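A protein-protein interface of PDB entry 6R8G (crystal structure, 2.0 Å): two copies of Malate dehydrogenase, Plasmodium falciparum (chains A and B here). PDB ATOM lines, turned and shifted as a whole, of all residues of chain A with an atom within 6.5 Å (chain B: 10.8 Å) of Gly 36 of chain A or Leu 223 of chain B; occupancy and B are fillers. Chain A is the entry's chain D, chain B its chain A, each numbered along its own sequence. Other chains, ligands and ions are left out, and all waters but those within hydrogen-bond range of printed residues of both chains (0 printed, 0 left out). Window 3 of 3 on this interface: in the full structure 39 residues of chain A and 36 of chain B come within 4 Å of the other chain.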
ATOM      1  N   VAL A  34     -33.444  18.436 -33.563  1.00  0.00           N
ATOM      2  CA  VAL A  34     -32.257  17.547 -33.748  1.00  0.00           C
ATOM      3  C   VAL A  34     -32.354  16.377 -32.773  1.00  0.00           C
ATOM      4  O   VAL A  34     -32.379  16.564 -31.561  1.00  0.00           O
ATOM      5  CB  VAL A  34     -30.915  18.283 -33.581  1.00  0.00           C
ATOM      6  CG1 VAL A  34     -29.728  17.336 -33.807  1.00  0.00           C
ATOM      7  CG2 VAL A  34     -30.848  19.497 -34.518  1.00  0.00           C
ATOM      8  N   PRO A  35     -32.427  15.142 -33.297  1.00  0.00           N
ATOM      9  CA  PRO A  35     -32.534  13.951 -32.470  1.00  0.00           C
ATOM     10  C   PRO A  35     -31.410  13.897 -31.429  1.00  0.00           C
ATOM     11  O   PRO A  35     -30.292  14.147 -31.757  1.00  0.00           O
ATOM     12  CB  PRO A  35     -32.438  12.801 -33.478  1.00  0.00           C
ATOM     13  CG  PRO A  35     -33.029  13.409 -34.722  1.00  0.00           C
ATOM     14  CD  PRO A  35     -32.465  14.824 -34.732  1.00  0.00           C
ATOM     15  N   GLY A  36     -31.757  13.619 -30.175  1.00  0.00           N
ATOM     16  CA  GLY A  36     -30.784  13.263 -29.127  1.00  0.00           C
ATOM     17  C   GLY A  36     -30.327  14.465 -28.314  1.00  0.00           C
ATOM     18  O   GLY A  36     -30.071  14.296 -27.109  1.00  0.00           O
ATOM     19  N   ILE A  37     -30.262  15.661 -28.908  1.00  0.00           N
ATOM     20  CA  ILE A  37     -29.695  16.848 -28.210  1.00  0.00           C
ATOM     21  C   ILE A  37     -30.504  17.121 -26.945  1.00  0.00           C
ATOM     22  O   ILE A  37     -29.916  17.203 -25.865  1.00  0.00           O
ATOM     23  CB  ILE A  37     -29.499  18.048 -29.155  1.00  0.00           C
ATOM     24  CG1 ILE A  37     -28.355  17.681 -30.126  1.00  0.00           C
ATOM     25  CG2 ILE A  37     -29.181  19.298 -28.379  1.00  0.00           C
ATOM     26  CD1 ILE A  37     -28.021  18.709 -31.139  1.00  0.00           C
ATOM     27  N   PRO A  38     -31.843  17.259 -27.008  1.00  0.00           N
ATOM     28  CA  PRO A  38     -32.601  17.579 -25.810  1.00  0.00           C
ATOM     29  C   PRO A  38     -32.575  16.435 -24.777  1.00  0.00           C
ATOM     30  O   PRO A  38     -32.539  16.725 -23.583  1.00  0.00           O
ATOM     31  CB  PRO A  38     -33.984  17.939 -26.330  1.00  0.00           C
ATOM     32  CG  PRO A  38     -34.087  17.303 -27.684  1.00  0.00           C
ATOM     33  CD  PRO A  38     -32.676  17.202 -28.208  1.00  0.00           C
ATOM     34  N   GLN A  39     -32.507  15.181 -25.243  1.00  0.00           N
ATOM     35  CA  GLN A  39     -32.415  13.977 -24.373  1.00  0.00           C
ATOM     36  C   GLN A  39     -31.113  14.058 -23.571  1.00  0.00           C
ATOM     37  O   GLN A  39     -31.152  13.828 -22.335  1.00  0.00           O
ATOM     38  CB  GLN A  39     -32.569  12.669 -25.166  1.00  0.00           C
ATOM     39  CG  GLN A  39     -33.950  12.449 -25.781  1.00  0.00           C
ATOM     40  CD  GLN A  39     -34.120  13.112 -27.142  1.00  0.00           C
ATOM     41  OE1 GLN A  39     -33.231  13.806 -27.640  1.00  0.00           O
ATOM     42  NE2 GLN A  39     -35.242  12.872 -27.800  1.00  0.00           N
ATOM     43  N   GLY A  40     -29.995  14.353 -24.231  1.00  0.00           N
ATOM     44  CA  GLY A  40     -28.667  14.444 -23.583  1.00  0.00           C
ATOM     45  C   GLY A  40     -28.615  15.558 -22.568  1.00  0.00           C
ATOM     46  O   GLY A  40     -28.136  15.325 -21.461  1.00  0.00           O
ATOM     47  N   LYS A  41     -29.081  16.744 -22.949  1.00  0.00           N
ATOM     48  CA  LYS A  41     -29.106  17.916 -22.054  1.00  0.00           C
ATOM     49  C   LYS A  41     -30.084  17.663 -20.898  1.00  0.00           C
ATOM     50  O   LYS A  41     -29.765  18.122 -19.791  1.00  0.00           O
ATOM     51  CB  LYS A  41     -29.449  19.181 -22.832  1.00  0.00           C
ATOM     52  CG  LYS A  41     -28.293  19.632 -23.696  1.00  0.00           C
ATOM     53  CD  LYS A  41     -28.460  20.908 -24.388  1.00  0.00           C
ATOM     54  CE  LYS A  41     -27.305  21.153 -25.338  1.00  0.00           C
ATOM     55  NZ  LYS A  41     -27.309  22.553 -25.744  1.00  0.00           N
ATOM     56  N   LEU A  43     -30.673  14.756 -19.490  1.00  0.00           N
ATOM     57  CA  LEU A  43     -29.892  13.874 -18.566  1.00  0.00           C
ATOM     58  C   LEU A  43     -28.970  14.748 -17.705  1.00  0.00           C
ATOM     59  O   LEU A  43     -28.989  14.628 -16.455  1.00  0.00           O
ATOM     60  CB  LEU A  43     -29.111  12.820 -19.334  1.00  0.00           C
ATOM     61  CG  LEU A  43     -29.951  11.684 -19.919  1.00  0.00           C
ATOM     62  CD1 LEU A  43     -29.114  10.839 -20.873  1.00  0.00           C
ATOM     63  CD2 LEU A  43     -30.540  10.779 -18.817  1.00  0.00           C
ATOM     64  N   ASN A  62     -38.060  15.186 -28.959  1.00  0.00           N
ATOM     65  CA  ASN A  62     -38.121  15.620 -30.365  1.00  0.00           C
ATOM     66  C   ASN A  62     -39.587  15.638 -30.811  1.00  0.00           C
ATOM     67  O   ASN A  62     -39.818  15.872 -32.017  1.00  0.00           O
ATOM     68  CB  ASN A  62     -37.265  14.704 -31.242  1.00  0.00           C
ATOM     69  CG  ASN A  62     -35.805  14.821 -30.888  1.00  0.00           C
ATOM     70  OD1 ASN A  62     -35.203  13.833 -30.474  1.00  0.00           O
ATOM     71  ND2 ASN A  62     -35.241  16.009 -30.999  1.00  0.00           N
ATOM     72  N   ARG B  81     -13.294  13.827 -24.792  1.00  0.00           N
ATOM     73  CA  ARG B  81     -13.589  12.630 -25.616  1.00  0.00           C
ATOM     74  C   ARG B  81     -14.883  12.888 -26.419  1.00  0.00           C
ATOM     75  O   ARG B  81     -15.848  13.485 -25.870  1.00  0.00           O
ATOM     76  CB  ARG B  81     -13.627  11.396 -24.692  1.00  0.00           C
ATOM     77  CG  ARG B  81     -14.657  11.434 -23.566  1.00  0.00           C
ATOM     78  CD  ARG B  81     -15.218  10.039 -23.410  1.00  0.00           C
ATOM     79  NE  ARG B  81     -16.192   9.871 -22.360  1.00  0.00           N
ATOM     80  CZ  ARG B  81     -16.768   8.715 -22.072  1.00  0.00           C
ATOM     81  NH1 ARG B  81     -17.661   8.637 -21.096  1.00  0.00           N
ATOM     82  NH2 ARG B  81     -16.445   7.631 -22.745  1.00  0.00           N
ATOM     83  N   LYS B  82     -14.914  12.453 -27.683  1.00  0.00           N
ATOM     84  CA  LYS B  82     -16.123  12.435 -28.548  1.00  0.00           C
ATOM     85  C   LYS B  82     -16.659  10.990 -28.613  1.00  0.00           C
ATOM     86  O   LYS B  82     -16.058  10.103 -27.975  1.00  0.00           O
ATOM     87  CB  LYS B  82     -15.759  13.020 -29.919  1.00  0.00           C
ATOM     88  CG  LYS B  82     -16.915  13.629 -30.707  1.00  0.00           C
ATOM     89  CD  LYS B  82     -17.531  14.872 -30.082  1.00  0.00           C
ATOM     90  CE  LYS B  82     -18.888  15.189 -30.670  1.00  0.00           C
ATOM     91  NZ  LYS B  82     -18.994  16.625 -31.030  1.00  0.00           N
ATOM     92  N   GLU B  83     -17.778  10.755 -29.309  1.00  0.00           N
ATOM     93  CA  GLU B  83     -18.437   9.417 -29.393  1.00  0.00           C
ATOM     94  C   GLU B  83     -17.488   8.455 -30.126  1.00  0.00           C
ATOM     95  O   GLU B  83     -16.946   8.858 -31.150  1.00  0.00           O
ATOM     96  CB  GLU B  83     -19.822   9.575 -30.029  1.00  0.00           C
ATOM     97  CG  GLU B  83     -20.710   8.356 -29.908  1.00  0.00           C
ATOM     98  CD  GLU B  83     -21.711   8.243 -31.055  1.00  0.00           C
ATOM     99  OE1 GLU B  83     -22.291   9.272 -31.478  1.00  0.00           O
ATOM    100  OE2 GLU B  83     -21.892   7.138 -31.540  1.00  0.00           O
ATOM    101  N   GLY B  84     -17.279   7.250 -29.595  1.00  0.00           N
ATOM    102  CA  GLY B  84     -16.351   6.232 -30.127  1.00  0.00           C
ATOM    103  C   GLY B  84     -15.071   6.154 -29.310  1.00  0.00           C
ATOM    104  O   GLY B  84     -14.338   5.165 -29.522  1.00  0.00           O
ATOM    105  N   LYS B 212     -26.104   1.774 -16.269  1.00  0.00           N
ATOM    106  CA  LYS B 212     -26.409   3.133 -16.770  1.00  0.00           C
ATOM    107  C   LYS B 212     -25.458   4.163 -16.164  1.00  0.00           C
ATOM    108  O   LYS B 212     -25.076   5.099 -16.881  1.00  0.00           O
ATOM    109  CB  LYS B 212     -27.843   3.515 -16.455  1.00  0.00           C
ATOM    110  CG  LYS B 212     -28.867   2.872 -17.367  1.00  0.00           C
ATOM    111  CD  LYS B 212     -30.211   3.028 -16.752  1.00  0.00           C
ATOM    112  CE  LYS B 212     -31.312   2.569 -17.672  1.00  0.00           C
ATOM    113  NZ  LYS B 212     -32.577   3.082 -17.127  1.00  0.00           N
ATOM    114  N   ASN B 215     -21.978   4.065 -17.883  1.00  0.00           N
ATOM    115  CA  ASN B 215     -22.074   4.379 -19.323  1.00  0.00           C
ATOM    116  C   ASN B 215     -22.635   5.792 -19.524  1.00  0.00           C
ATOM    117  O   ASN B 215     -22.725   6.193 -20.675  1.00  0.00           O
ATOM    118  CB  ASN B 215     -22.888   3.314 -20.072  1.00  0.00           C
ATOM    119  CG  ASN B 215     -22.175   1.976 -20.122  1.00  0.00           C
ATOM    120  OD1 ASN B 215     -20.955   1.899 -20.278  1.00  0.00           O
ATOM    121  ND2 ASN B 215     -22.919   0.893 -19.954  1.00  0.00           N
ATOM    122  N   MET B 216     -22.934   6.540 -18.462  1.00  0.00           N
ATOM    123  CA  MET B 216     -23.718   7.805 -18.567  1.00  0.00           C
ATOM    124  C   MET B 216     -22.958   8.839 -19.370  1.00  0.00           C
ATOM    125  O   MET B 216     -23.587   9.523 -20.242  1.00  0.00           O
ATOM    126  CB  MET B 216     -24.088   8.407 -17.199  1.00  0.00           C
ATOM    127  CG  MET B 216     -25.105   9.487 -17.276  1.00  0.00           C
ATOM    128  SD  MET B 216     -26.661   8.957 -18.082  1.00  0.00           S
ATOM    129  CE  MET B 216     -27.534   8.200 -16.729  1.00  0.00           C
ATOM    130  N   GLY B 217     -21.684   9.021 -19.059  1.00  0.00           N
ATOM    131  CA  GLY B 217     -20.853   9.986 -19.801  1.00  0.00           C
ATOM    132  C   GLY B 217     -20.882   9.722 -21.305  1.00  0.00           C
ATOM    133  O   GLY B 217     -21.097  10.677 -22.053  1.00  0.00           O
ATOM    134  N   ALA B 218     -20.707   8.479 -21.731  1.00  0.00           N
ATOM    135  CA  ALA B 218     -20.714   8.098 -23.162  1.00  0.00           C
ATOM    136  C   ALA B 218     -22.130   8.312 -23.722  1.00  0.00           C
ATOM    137  O   ALA B 218     -22.233   8.721 -24.897  1.00  0.00           O
ATOM    138  CB  ALA B 218     -20.224   6.673 -23.342  1.00  0.00           C
ATOM    139  N   GLU B 219     -23.179   8.061 -22.924  1.00  0.00           N
ATOM    140  CA  GLU B 219     -24.587   8.183 -23.408  1.00  0.00           C
ATOM    141  C   GLU B 219     -24.898   9.660 -23.676  1.00  0.00           C
ATOM    142  O   GLU B 219     -25.447   9.970 -24.727  1.00  0.00           O
ATOM    143  CB  GLU B 219     -25.618   7.580 -22.448  1.00  0.00           C
ATOM    144  CG  GLU B 219     -26.923   7.214 -23.185  1.00  0.00           C
ATOM    145  CD  GLU B 219     -28.177   7.030 -22.338  1.00  0.00           C
ATOM    146  OE1 GLU B 219     -28.054   6.919 -21.084  1.00  0.00           O
ATOM    147  OE2 GLU B 219     -29.283   6.958 -22.943  1.00  0.00           O
ATOM    148  N   ILE B 220     -24.476  10.543 -22.793  1.00  0.00           N
ATOM    149  CA  ILE B 220     -24.675  12.007 -22.961  1.00  0.00           C
ATOM    150  C   ILE B 220     -23.901  12.460 -24.202  1.00  0.00           C
ATOM    151  O   ILE B 220     -24.451  13.241 -24.972  1.00  0.00           O
ATOM    152  CB  ILE B 220     -24.275  12.769 -21.696  1.00  0.00           C
ATOM    153  CG1 ILE B 220     -25.252  12.450 -20.567  1.00  0.00           C
ATOM    154  CG2 ILE B 220     -24.159  14.267 -21.973  1.00  0.00           C
ATOM    155  CD1 ILE B 220     -24.897  13.126 -19.230  1.00  0.00           C
ATOM    156  N   ILE B 221     -22.658  11.996 -24.365  1.00  0.00           N
ATOM    157  CA  ILE B 221     -21.837  12.350 -25.551  1.00  0.00           C
ATOM    158  C   ILE B 221     -22.594  11.867 -26.800  1.00  0.00           C
ATOM    159  O   ILE B 221     -22.669  12.640 -27.769  1.00  0.00           O
ATOM    160  CB  ILE B 221     -20.404  11.784 -25.461  1.00  0.00           C
ATOM    161  CG1 ILE B 221     -19.572  12.564 -24.429  1.00  0.00           C
ATOM    162  CG2 ILE B 221     -19.766  11.762 -26.857  1.00  0.00           C
ATOM    163  CD1 ILE B 221     -18.288  11.898 -24.022  1.00  0.00           C
ATOM    164  N   LYS B 222     -23.154  10.660 -26.767  1.00  0.00           N
ATOM    165  CA  LYS B 222     -23.842  10.060 -27.936  1.00  0.00           C
ATOM    166  C   LYS B 222     -25.098  10.859 -28.283  1.00  0.00           C
ATOM    167  O   LYS B 222     -25.381  10.986 -29.451  1.00  0.00           O
ATOM    168  CB  LYS B 222     -24.227   8.599 -27.684  1.00  0.00           C
ATOM    169  CG  LYS B 222     -24.868   7.930 -28.883  1.00  0.00           C
ATOM    170  CD  LYS B 222     -25.210   6.471 -28.663  1.00  0.00           C
ATOM    171  CE  LYS B 222     -25.866   5.900 -29.904  1.00  0.00           C
ATOM    172  NZ  LYS B 222     -26.228   4.463 -29.751  1.00  0.00           N
ATOM    173  N   LEU B 223     -25.837  11.371 -27.303  1.00  0.00           N
ATOM    174  CA  LEU B 223     -27.134  12.059 -27.517  1.00  0.00           C
ATOM    175  C   LEU B 223     -26.905  13.554 -27.806  1.00  0.00           C
ATOM    176  O   LEU B 223     -27.487  14.093 -28.739  1.00  0.00           O
ATOM    177  CB  LEU B 223     -27.964  11.880 -26.245  1.00  0.00           C
ATOM    178  CG  LEU B 223     -28.505  10.484 -25.974  1.00  0.00           C
ATOM    179  CD1 LEU B 223     -29.108  10.433 -24.563  1.00  0.00           C
ATOM    180  CD2 LEU B 223     -29.521  10.046 -27.044  1.00  0.00           C
ATOM    181  N   ALA B 224     -26.133  14.220 -26.976  1.00  0.00           N
ATOM    182  CA  ALA B 224     -25.947  15.679 -26.995  1.00  0.00           C
ATOM    183  C   ALA B 224     -24.787  16.062 -27.928  1.00  0.00           C
ATOM    184  O   ALA B 224     -24.588  17.261 -28.118  1.00  0.00           O
ATOM    185  CB  ALA B 224     -25.682  16.153 -25.571  1.00  0.00           C
ATOM    186  N   LYS B 225     -24.018  15.114 -28.456  1.00  0.00           N
ATOM    187  CA  LYS B 225     -22.818  15.408 -29.299  1.00  0.00           C
ATOM    188  C   LYS B 225     -21.847  16.332 -28.546  1.00  0.00           C
ATOM    189  O   LYS B 225     -21.155  17.123 -29.194  1.00  0.00           O
ATOM    190  CB  LYS B 225     -23.235  16.072 -30.622  1.00  0.00           C
ATOM    191  CG  LYS B 225     -24.118  15.215 -31.507  1.00  0.00           C
ATOM    192  CD  LYS B 225     -24.621  15.975 -32.710  1.00  0.00           C
ATOM    193  CE  LYS B 225     -25.724  15.228 -33.444  1.00  0.00           C
ATOM    194  NZ  LYS B 225     -26.603  16.187 -34.143  1.00  0.00           N
ATOM    195  N   ALA B 226     -21.799  16.236 -27.223  1.00  0.00           N
ATOM    196  CA  ALA B 226     -20.943  17.045 -26.328  1.00  0.00           C
ATOM    197  C   ALA B 226     -20.929  16.349 -24.956  1.00  0.00           C
ATOM    198  O   ALA B 226     -21.895  15.635 -24.648  1.00  0.00           O
ATOM    199  CB  ALA B 226     -21.475  18.460 -26.234  1.00  0.00           C
ATOM    200  N   SER B 227     -19.864  16.499 -24.186  1.00  0.00           N
ATOM    201  CA  SER B 227     -19.767  15.863 -22.865  1.00  0.00           C
ATOM    202  C   SER B 227     -20.576  16.722 -21.878  1.00  0.00           C
ATOM    203  O   SER B 227     -20.880  17.901 -22.164  1.00  0.00           O
ATOM    204  CB  SER B 227     -18.344  15.621 -22.418  1.00  0.00           C
ATOM    205  OG  SER B 227     -17.541  16.738 -22.713  1.00  0.00           O
ATOM    206  N   ALA B 228     -20.985  16.067 -20.816  1.00  0.00           N
ATOM    207  CA  ALA B 228     -21.744  16.662 -19.719  1.00  0.00           C
ATOM    208  C   ALA B 228     -21.059  17.962 -19.275  1.00  0.00           C
ATOM    209  O   ALA B 228     -19.847  18.001 -19.234  1.00  0.00           O
ATOM    210  CB  ALA B 228     -21.836  15.608 -18.642  1.00  0.00           C
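O of Leu 223 of chain B lies close to O of Gly 36 of chain A (3.1 Å).
The backbone carbonyl oxygen (O) of Leu 223 of chain B lies within hydrogen-bond range of the backbone NH (N) of Ile 37 of chain A, 3.2 Å away.
N of Gly 36 of chain A is in hydrogen-bond range of OD1 of Asn 62 of chain A.
NZ of Lys 82 of chain B is in hydrogen-bond range of O of Lys 225 of chain B.
OE1 of Gln 39 of chain A lies close to N of Gly 36 of chain A (2.9 Å).
The backbone carbonyl oxygen of Val 34 of chain A sits at hydrogen-bond distance from the side-chain amide nitrogen of Asn 62 of chain A, 3.0 Å away.
Among the printed residues, pairs that only touch across the chains: Val 34 of chain A with Lys 225 of chain B, Leu 43 of chain A with Leu 223 of chain B, Gly 40 of chain A with Leu 223 of chain B, Gly 36 of chain A with Ala 224 of chain B and Gly 40 of chain A with Ala 224 of chain B.
Printed residues of chain B within 4 Å of Gly 36 of chain A: Leu 223 (2.9 Å) and Ala 224 (3.9 Å).
Of chain A, only Gly 36 (2.9 Å), Ile 37 (3.2 Å), Gly 40 (3.8 Å) and Leu 43 (3.7 Å) come within 4 Å of Leu 223 of chain B.
No residue of chain B comes within 4 Å of Pro 35 of chain A.
Of chain B, only Leu 223 comes within 4 Å of Ile 37 of chain A.
Of chain B, only Leu 223 (3.8 Å) and Ala 224 (3.97 Å) come within 4 Å of Gly 40 of chain A.
Of the printed residues of chain B, Val 34 of chain A touches Lys 225.
Of the printed residues of chain A, Ala 224 of chain B touches Gly 36 and Gly 40.
Asn 215 of chain B touches none of the printed residues of chain A.
Hydrophobic or aromatic side chains of chain B within 4 Å of the printed part of chain A: Leu 223 and Ala 224.
Of the 10 printed residues of chain A, 5 touch a printed residue of chain B.
Printed residues of chain A that touch a printed residue of chain B: Val 34, Gly 36, Ile 37, Gly 40 and Leu 43.
Hydrophobic or aromatic side chains of chain A within 4 Å of the printed part of chain B: Val 34, Ile 37 and Leu 43.
Along chain A the printed residues that touch a printed residue of chain B span positions 34 to 43.
Among the printed residues, 7 pairs touch across the chains.
Among the printed residues, no Asp or Glu carboxylate lies within 4 Å of a Lys or Arg side-chain nitrogen of the other chain.
No position is printed for both chains.
Of the 7 pairs that touch across the chains among the printed residues, none has its exchanged pair printed and touching as well.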
